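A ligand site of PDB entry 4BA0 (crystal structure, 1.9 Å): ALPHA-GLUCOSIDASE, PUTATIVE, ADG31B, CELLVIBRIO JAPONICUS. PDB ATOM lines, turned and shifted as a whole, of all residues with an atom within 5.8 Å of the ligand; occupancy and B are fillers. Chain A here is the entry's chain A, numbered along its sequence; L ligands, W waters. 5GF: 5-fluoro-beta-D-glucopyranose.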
ATOM      1  N   TYR A 189      23.408   9.493  21.356  1.00  0.00           N
ATOM      2  CA  TYR A 189      23.109   8.405  22.285  1.00  0.00           C
ATOM      3  C   TYR A 189      24.308   7.575  22.693  1.00  0.00           C
ATOM      4  O   TYR A 189      24.453   7.180  23.839  1.00  0.00           O
ATOM      5  CB  TYR A 189      22.076   7.456  21.638  1.00  0.00           C
ATOM      6  CG  TYR A 189      20.872   8.200  21.119  1.00  0.00           C
ATOM      7  CD1 TYR A 189      19.777   8.431  21.944  1.00  0.00           C
ATOM      8  CD2 TYR A 189      20.840   8.711  19.829  1.00  0.00           C
ATOM      9  CE1 TYR A 189      18.689   9.141  21.500  1.00  0.00           C
ATOM     10  CE2 TYR A 189      19.749   9.412  19.363  1.00  0.00           C
ATOM     11  CZ  TYR A 189      18.679   9.622  20.207  1.00  0.00           C
ATOM     12  OH  TYR A 189      17.571  10.319  19.781  1.00  0.00           O
ATOM     13  N   ARG A 270       6.891  -0.451  15.387  1.00  0.00           N
ATOM     14  CA  ARG A 270       6.423   0.937  15.410  1.00  0.00           C
ATOM     15  C   ARG A 270       6.440   1.389  16.870  1.00  0.00           C
ATOM     16  O   ARG A 270       6.581   0.584  17.790  1.00  0.00           O
ATOM     17  CB  ARG A 270       5.000   1.077  14.877  1.00  0.00           C
ATOM     18  CG  ARG A 270       3.969   0.254  15.673  1.00  0.00           C
ATOM     19  CD  ARG A 270       2.533   0.534  15.249  1.00  0.00           C
ATOM     20  NE  ARG A 270       2.362   0.433  13.800  1.00  0.00           N
ATOM     21  CZ  ARG A 270       1.413   1.049  13.104  1.00  0.00           C
ATOM     22  NH1 ARG A 270       0.524   1.806  13.732  1.00  0.00           N
ATOM     23  NH2 ARG A 270       1.358   0.924  11.782  1.00  0.00           N
ATOM     24  N   PHE A 271       6.281   2.686  17.091  1.00  0.00           N
ATOM     25  CA  PHE A 271       6.018   3.205  18.422  1.00  0.00           C
ATOM     26  C   PHE A 271       4.581   3.712  18.369  1.00  0.00           C
ATOM     27  O   PHE A 271       4.368   4.868  17.990  1.00  0.00           O
ATOM     28  CB  PHE A 271       6.987   4.353  18.727  1.00  0.00           C
ATOM     29  CG  PHE A 271       6.684   5.103  20.022  1.00  0.00           C
ATOM     30  CD1 PHE A 271       5.940   4.525  21.035  1.00  0.00           C
ATOM     31  CD2 PHE A 271       7.170   6.384  20.195  1.00  0.00           C
ATOM     32  CE1 PHE A 271       5.679   5.234  22.228  1.00  0.00           C
ATOM     33  CE2 PHE A 271       6.926   7.106  21.384  1.00  0.00           C
ATOM     34  CZ  PHE A 271       6.178   6.511  22.396  1.00  0.00           C
ATOM     35  N   ASP A 299       6.566  -1.872  21.711  1.00  0.00           N
ATOM     36  CA  ASP A 299       7.003  -0.681  22.419  1.00  0.00           C
ATOM     37  C   ASP A 299       6.231  -0.536  23.724  1.00  0.00           C
ATOM     38  O   ASP A 299       5.583  -1.495  24.178  1.00  0.00           O
ATOM     39  CB  ASP A 299       6.780   0.545  21.511  1.00  0.00           C
ATOM     40  CG  ASP A 299       7.788   1.645  21.749  1.00  0.00           C
ATOM     41  OD1 ASP A 299       8.047   1.999  22.924  1.00  0.00           O
ATOM     42  OD2 ASP A 299       8.329   2.185  20.745  1.00  0.00           O
ATOM     43  N   LEU A 300       6.294   0.637  24.336  1.00  0.00           N
ATOM     44  CA  LEU A 300       5.910   0.782  25.746  1.00  0.00           C
ATOM     45  C   LEU A 300       4.427   0.576  26.077  1.00  0.00           C
ATOM     46  O   LEU A 300       4.058   0.540  27.256  1.00  0.00           O
ATOM     47  CB  LEU A 300       6.420   2.098  26.340  1.00  0.00           C
ATOM     48  CG  LEU A 300       6.108   3.389  25.576  1.00  0.00           C
ATOM     49  CD1 LEU A 300       4.604   3.657  25.513  1.00  0.00           C
ATOM     50  CD2 LEU A 300       6.845   4.574  26.231  1.00  0.00           C
ATOM     51  N   ILE A 341      10.127  -4.031  24.766  1.00  0.00           N
ATOM     52  CA  ILE A 341      10.928  -2.926  25.265  1.00  0.00           C
ATOM     53  C   ILE A 341      10.974  -2.916  26.813  1.00  0.00           C
ATOM     54  O   ILE A 341      10.003  -3.290  27.487  1.00  0.00           O
ATOM     55  CB  ILE A 341      10.384  -1.579  24.745  1.00  0.00           C
ATOM     56  CG1 ILE A 341      11.446  -0.487  24.870  1.00  0.00           C
ATOM     57  CG2 ILE A 341       9.105  -1.181  25.495  1.00  0.00           C
ATOM     58  CD1 ILE A 341      11.015   0.835  24.238  1.00  0.00           C
ATOM     59  N   GLU A 343      13.125  -0.400  30.091  1.00  0.00           N
ATOM     60  CA  GLU A 343      13.853   0.829  30.331  1.00  0.00           C
ATOM     61  C   GLU A 343      14.485   0.763  31.727  1.00  0.00           C
ATOM     62  O   GLU A 343      14.106  -0.065  32.542  1.00  0.00           O
ATOM     63  CB  GLU A 343      12.894   2.019  30.242  1.00  0.00           C
ATOM     64  CG  GLU A 343      12.317   2.268  28.844  1.00  0.00           C
ATOM     65  CD  GLU A 343      10.949   1.652  28.624  1.00  0.00           C
ATOM     66  OE1 GLU A 343      10.491   0.875  29.485  1.00  0.00           O
ATOM     67  OE2 GLU A 343      10.321   1.940  27.578  1.00  0.00           O
ATOM     68  N   PHE A 377       8.432  10.914  31.460  1.00  0.00           N
ATOM     69  CA  PHE A 377       7.352   9.961  31.737  1.00  0.00           C
ATOM     70  C   PHE A 377       6.744  10.112  33.133  1.00  0.00           C
ATOM     71  O   PHE A 377       5.709   9.519  33.425  1.00  0.00           O
ATOM     72  CB  PHE A 377       7.884   8.537  31.530  1.00  0.00           C
ATOM     73  CG  PHE A 377       8.644   8.359  30.236  1.00  0.00           C
ATOM     74  CD1 PHE A 377       7.968   8.036  29.060  1.00  0.00           C
ATOM     75  CD2 PHE A 377      10.011   8.548  30.188  1.00  0.00           C
ATOM     76  CE1 PHE A 377       8.669   7.886  27.872  1.00  0.00           C
ATOM     77  CE2 PHE A 377      10.701   8.402  28.991  1.00  0.00           C
ATOM     78  CZ  PHE A 377      10.037   8.069  27.831  1.00  0.00           C
ATOM     79  N   TRP A 410      14.670  -5.425  24.122  1.00  0.00           N
ATOM     80  CA  TRP A 410      14.973  -4.107  23.593  1.00  0.00           C
ATOM     81  C   TRP A 410      15.146  -3.251  24.831  1.00  0.00           C
ATOM     82  O   TRP A 410      14.230  -3.169  25.653  1.00  0.00           O
ATOM     83  CB  TRP A 410      13.779  -3.646  22.761  1.00  0.00           C
ATOM     84  CG  TRP A 410      13.861  -2.270  22.156  1.00  0.00           C
ATOM     85  CD1 TRP A 410      14.957  -1.472  22.035  1.00  0.00           C
ATOM     86  CD2 TRP A 410      12.763  -1.537  21.596  1.00  0.00           C
ATOM     87  NE1 TRP A 410      14.616  -0.285  21.400  1.00  0.00           N
ATOM     88  CE2 TRP A 410      13.276  -0.303  21.135  1.00  0.00           C
ATOM     89  CE3 TRP A 410      11.400  -1.814  21.421  1.00  0.00           C
ATOM     90  CZ2 TRP A 410      12.473   0.662  20.514  1.00  0.00           C
ATOM     91  CZ3 TRP A 410      10.600  -0.855  20.793  1.00  0.00           C
ATOM     92  CH2 TRP A 410      11.148   0.360  20.351  1.00  0.00           C
ATOM     93  N   ASP A 412      15.766   0.454  25.965  1.00  0.00           N
ATOM     94  CA  ASP A 412      15.751   1.847  25.517  1.00  0.00           C
ATOM     95  C   ASP A 412      16.148   2.790  26.649  1.00  0.00           C
ATOM     96  O   ASP A 412      15.993   2.445  27.819  1.00  0.00           O
ATOM     97  CB  ASP A 412      14.344   2.202  25.020  1.00  0.00           C
ATOM     98  CG  ASP A 412      14.329   3.416  24.109  1.00  0.00           C
ATOM     99  OD1 ASP A 412      15.409   3.949  23.793  1.00  0.00           O
ATOM    100  OD2 ASP A 412      13.223   3.816  23.704  1.00  0.00           O
ATOM    101  N   LEU A 413      16.675   3.964  26.282  1.00  0.00           N
ATOM    102  CA  LEU A 413      17.003   5.036  27.241  1.00  0.00           C
ATOM    103  C   LEU A 413      18.197   4.749  28.171  1.00  0.00           C
ATOM    104  O   LEU A 413      18.285   5.333  29.259  1.00  0.00           O
ATOM    105  CB  LEU A 413      15.782   5.404  28.093  1.00  0.00           C
ATOM    106  CG  LEU A 413      14.403   5.450  27.422  1.00  0.00           C
ATOM    107  CD1 LEU A 413      13.332   5.792  28.447  1.00  0.00           C
ATOM    108  CD2 LEU A 413      14.374   6.428  26.244  1.00  0.00           C
ATOM    109  N   ARG A 463      20.522   1.295  23.023  1.00  0.00           N
ATOM    110  CA  ARG A 463      20.764   2.605  22.428  1.00  0.00           C
ATOM    111  C   ARG A 463      22.111   3.213  22.852  1.00  0.00           C
ATOM    112  O   ARG A 463      22.624   4.158  22.212  1.00  0.00           O
ATOM    113  CB  ARG A 463      19.666   3.534  22.933  1.00  0.00           C
ATOM    114  CG  ARG A 463      19.255   4.607  21.990  1.00  0.00           C
ATOM    115  CD  ARG A 463      17.925   5.188  22.421  1.00  0.00           C
ATOM    116  NE  ARG A 463      18.040   6.111  23.551  1.00  0.00           N
ATOM    117  CZ  ARG A 463      17.123   7.041  23.806  1.00  0.00           C
ATOM    118  NH1 ARG A 463      16.056   7.107  23.020  1.00  0.00           N
ATOM    119  NH2 ARG A 463      17.261   7.887  24.830  1.00  0.00           N
ATOM    120  N   TRP A 477      21.156   0.738  17.725  1.00  0.00           N
ATOM    121  CA  TRP A 477      20.555   1.458  16.600  1.00  0.00           C
ATOM    122  C   TRP A 477      20.750   2.957  16.846  1.00  0.00           C
ATOM    123  O   TRP A 477      21.004   3.374  17.986  1.00  0.00           O
ATOM    124  CB  TRP A 477      19.080   1.091  16.440  1.00  0.00           C
ATOM    125  CG  TRP A 477      18.165   1.862  17.322  1.00  0.00           C
ATOM    126  CD1 TRP A 477      17.405   2.940  16.983  1.00  0.00           C
ATOM    127  CD2 TRP A 477      17.896   1.596  18.698  1.00  0.00           C
ATOM    128  NE1 TRP A 477      16.679   3.377  18.059  1.00  0.00           N
ATOM    129  CE2 TRP A 477      16.973   2.575  19.140  1.00  0.00           C
ATOM    130  CE3 TRP A 477      18.354   0.643  19.623  1.00  0.00           C
ATOM    131  CZ2 TRP A 477      16.492   2.617  20.453  1.00  0.00           C
ATOM    132  CZ3 TRP A 477      17.881   0.695  20.931  1.00  0.00           C
ATOM    133  CH2 TRP A 477      16.965   1.675  21.330  1.00  0.00           C
ATOM    134  N   GLY A 479      19.126   5.624  17.273  1.00  0.00           N
ATOM    135  CA  GLY A 479      18.212   6.503  17.993  1.00  0.00           C
ATOM    136  C   GLY A 479      17.102   7.150  17.172  1.00  0.00           C
ATOM    137  O   GLY A 479      16.745   6.662  16.093  1.00  0.00           O
ATOM    138  N   ASP A 480      16.573   8.256  17.687  1.00  0.00           N
ATOM    139  CA  ASP A 480      15.334   8.862  17.209  1.00  0.00           C
ATOM    140  C   ASP A 480      15.582   9.814  16.033  1.00  0.00           C
ATOM    141  O   ASP A 480      15.361  11.011  16.126  1.00  0.00           O
ATOM    142  CB  ASP A 480      14.617   9.581  18.358  1.00  0.00           C
ATOM    143  CG  ASP A 480      14.132   8.614  19.446  1.00  0.00           C
ATOM    144  OD1 ASP A 480      14.121   7.387  19.207  1.00  0.00           O
ATOM    145  OD2 ASP A 480      13.765   9.076  20.559  1.00  0.00           O
ATOM    146  N   ASP A 509      16.567   3.120  12.454  1.00  0.00           N
ATOM    147  CA  ASP A 509      15.129   2.968  12.342  1.00  0.00           C
ATOM    148  C   ASP A 509      14.784   3.197  10.874  1.00  0.00           C
ATOM    149  O   ASP A 509      14.720   4.333  10.411  1.00  0.00           O
ATOM    150  CB  ASP A 509      14.402   4.090  13.112  1.00  0.00           C
ATOM    151  CG  ASP A 509      14.429   3.898  14.609  1.00  0.00           C
ATOM    152  OD1 ASP A 509      14.799   2.814  15.115  1.00  0.00           O
ATOM    153  OD2 ASP A 509      14.053   4.881  15.289  1.00  0.00           O
ATOM    154  N   PHE A 513      12.216   7.947  12.174  1.00  0.00           N
ATOM    155  CA  PHE A 513      11.446   7.777  13.400  1.00  0.00           C
ATOM    156  C   PHE A 513      10.632   8.978  13.829  1.00  0.00           C
ATOM    157  O   PHE A 513       9.445   8.857  14.137  1.00  0.00           O
ATOM    158  CB  PHE A 513      12.399   7.430  14.548  1.00  0.00           C
ATOM    159  CG  PHE A 513      11.728   7.379  15.900  1.00  0.00           C
ATOM    160  CD1 PHE A 513      11.118   6.217  16.347  1.00  0.00           C
ATOM    161  CD2 PHE A 513      11.711   8.495  16.720  1.00  0.00           C
ATOM    162  CE1 PHE A 513      10.504   6.174  17.602  1.00  0.00           C
ATOM    163  CE2 PHE A 513      11.105   8.463  17.968  1.00  0.00           C
ATOM    164  CZ  PHE A 513      10.496   7.301  18.416  1.00  0.00           C
ATOM    165  N   ARG A 538      14.993  -3.324  10.341  1.00  0.00           N
ATOM    166  CA  ARG A 538      13.994  -2.929  11.337  1.00  0.00           C
ATOM    167  C   ARG A 538      13.439  -1.535  11.045  1.00  0.00           C
ATOM    168  O   ARG A 538      13.901  -0.534  11.609  1.00  0.00           O
ATOM    169  CB  ARG A 538      14.584  -2.972  12.749  1.00  0.00           C
ATOM    170  CG  ARG A 538      13.607  -2.684  13.903  1.00  0.00           C
ATOM    171  CD  ARG A 538      14.348  -2.722  15.296  1.00  0.00           C
ATOM    172  NE  ARG A 538      15.395  -1.730  15.201  1.00  0.00           N
ATOM    173  CZ  ARG A 538      15.183  -0.430  15.406  1.00  0.00           C
ATOM    174  NH1 ARG A 538      13.983  -0.023  15.804  1.00  0.00           N
ATOM    175  NH2 ARG A 538      16.159   0.445  15.211  1.00  0.00           N
ATOM    176  N   HIS A 540      11.014   1.351  11.779  1.00  0.00           N
ATOM    177  CA  HIS A 540      10.455   1.754  13.074  1.00  0.00           C
ATOM    178  C   HIS A 540      10.222   3.243  13.087  1.00  0.00           C
ATOM    179  O   HIS A 540      11.095   4.002  12.658  1.00  0.00           O
ATOM    180  CB  HIS A 540      11.441   1.387  14.184  1.00  0.00           C
ATOM    181  CG  HIS A 540      10.998   1.794  15.548  1.00  0.00           C
ATOM    182  ND1 HIS A 540       9.916   1.232  16.185  1.00  0.00           N
ATOM    183  CD2 HIS A 540      11.529   2.685  16.428  1.00  0.00           C
ATOM    184  CE1 HIS A 540       9.788   1.756  17.402  1.00  0.00           C
ATOM    185  NE2 HIS A 540      10.751   2.644  17.570  1.00  0.00           N
HETATM  186  O5  5GF L   1      11.884   5.565  23.152  1.00  0.00           O
HETATM  187  C1  5GF L   1      13.156   4.920  22.947  1.00  0.00           C
HETATM  188  F   5GF L   1      10.497   6.434  21.625  1.00  0.00           F
HETATM  189  C2  5GF L   1      13.571   4.643  21.488  1.00  0.00           C
HETATM  190  O2  5GF L   1      14.592   5.540  21.043  1.00  0.00           O
HETATM  191  C3  5GF L   1      12.400   4.668  20.513  1.00  0.00           C
HETATM  192  O3  5GF L   1      12.674   3.786  19.404  1.00  0.00           O
HETATM  193  C4  5GF L   1      11.157   4.219  21.241  1.00  0.00           C
HETATM  194  O4  5GF L   1      10.092   4.005  20.313  1.00  0.00           O
HETATM  195  C6  5GF L   1       9.558   4.900  23.064  1.00  0.00           C
HETATM  196  O6  5GF L   1       9.812   3.716  23.828  1.00  0.00           O
HETATM  197  C5  5GF L   1      10.788   5.297  22.261  1.00  0.00           C
HETATM  198  O   HOH W   1      14.306   5.027  17.811  1.00  0.00           O
HETATM  199  O   HOH W   2      13.534   8.362  23.506  1.00  0.00           O
HETATM  200  O   HOH W   3      11.137   3.874  26.179  1.00  0.00           O
HETATM  201  O   HOH W   4      11.297   9.423  21.740  1.00  0.00           O
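The side-chain carboxylate of Asp 412 is bonded to a carbon (C1) of the ligand (1.3 Å). The side-chain carboxylate of Asp 299 sits at hydrogen-bond distance from an oxygen (O4) of the ligand, 2.6 Å away. The side-chain carboxylate (OD1) of Asp 480 is in hydrogen-bond range of an oxygen (O2) of the ligand, 2.6 Å away. A ring nitrogen (NE2) of His 540 lies within hydrogen-bond range of an oxygen (O3) of the ligand (2.9 Å). O2 of the ligand is in hydrogen-bond range of NH1 of Arg 463 (2.9 Å).
NH1 of Arg 463 is in salt-bridge range of OD1 of Asp 412. OD2 of Asp 480 lies within salt-bridge range of NH1 of Arg 463 (3.9 Å). N of Asp 480 lies within hydrogen-bond range of OH of Tyr 189 (3.1 Å).
Phe 271 touches the ligand (CB to O4, 3.5 Å). CD2 of Leu 300 touches O6 of the ligand (3.9 Å). Ile 341 touches the ligand (CD1 to O6, 3.1 Å). CZ2 of Trp 410 touches O3 of the ligand (3.3 Å). Leu 413 touches the ligand (CD2 to C1, 3.8 Å). Trp 477 touches the ligand. CZ of Phe 513 touches F of the ligand, at 3.3 Å.
Water W3 lies within hydrogen-bond range of OE2 of Glu 343, O6 of the ligand and OD2 of Asp 412. Water W2 lies within hydrogen-bond range of the guanidinium group of Arg 463, the side-chain carboxylate of Asp 480 and an oxygen (O5) of the ligand.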
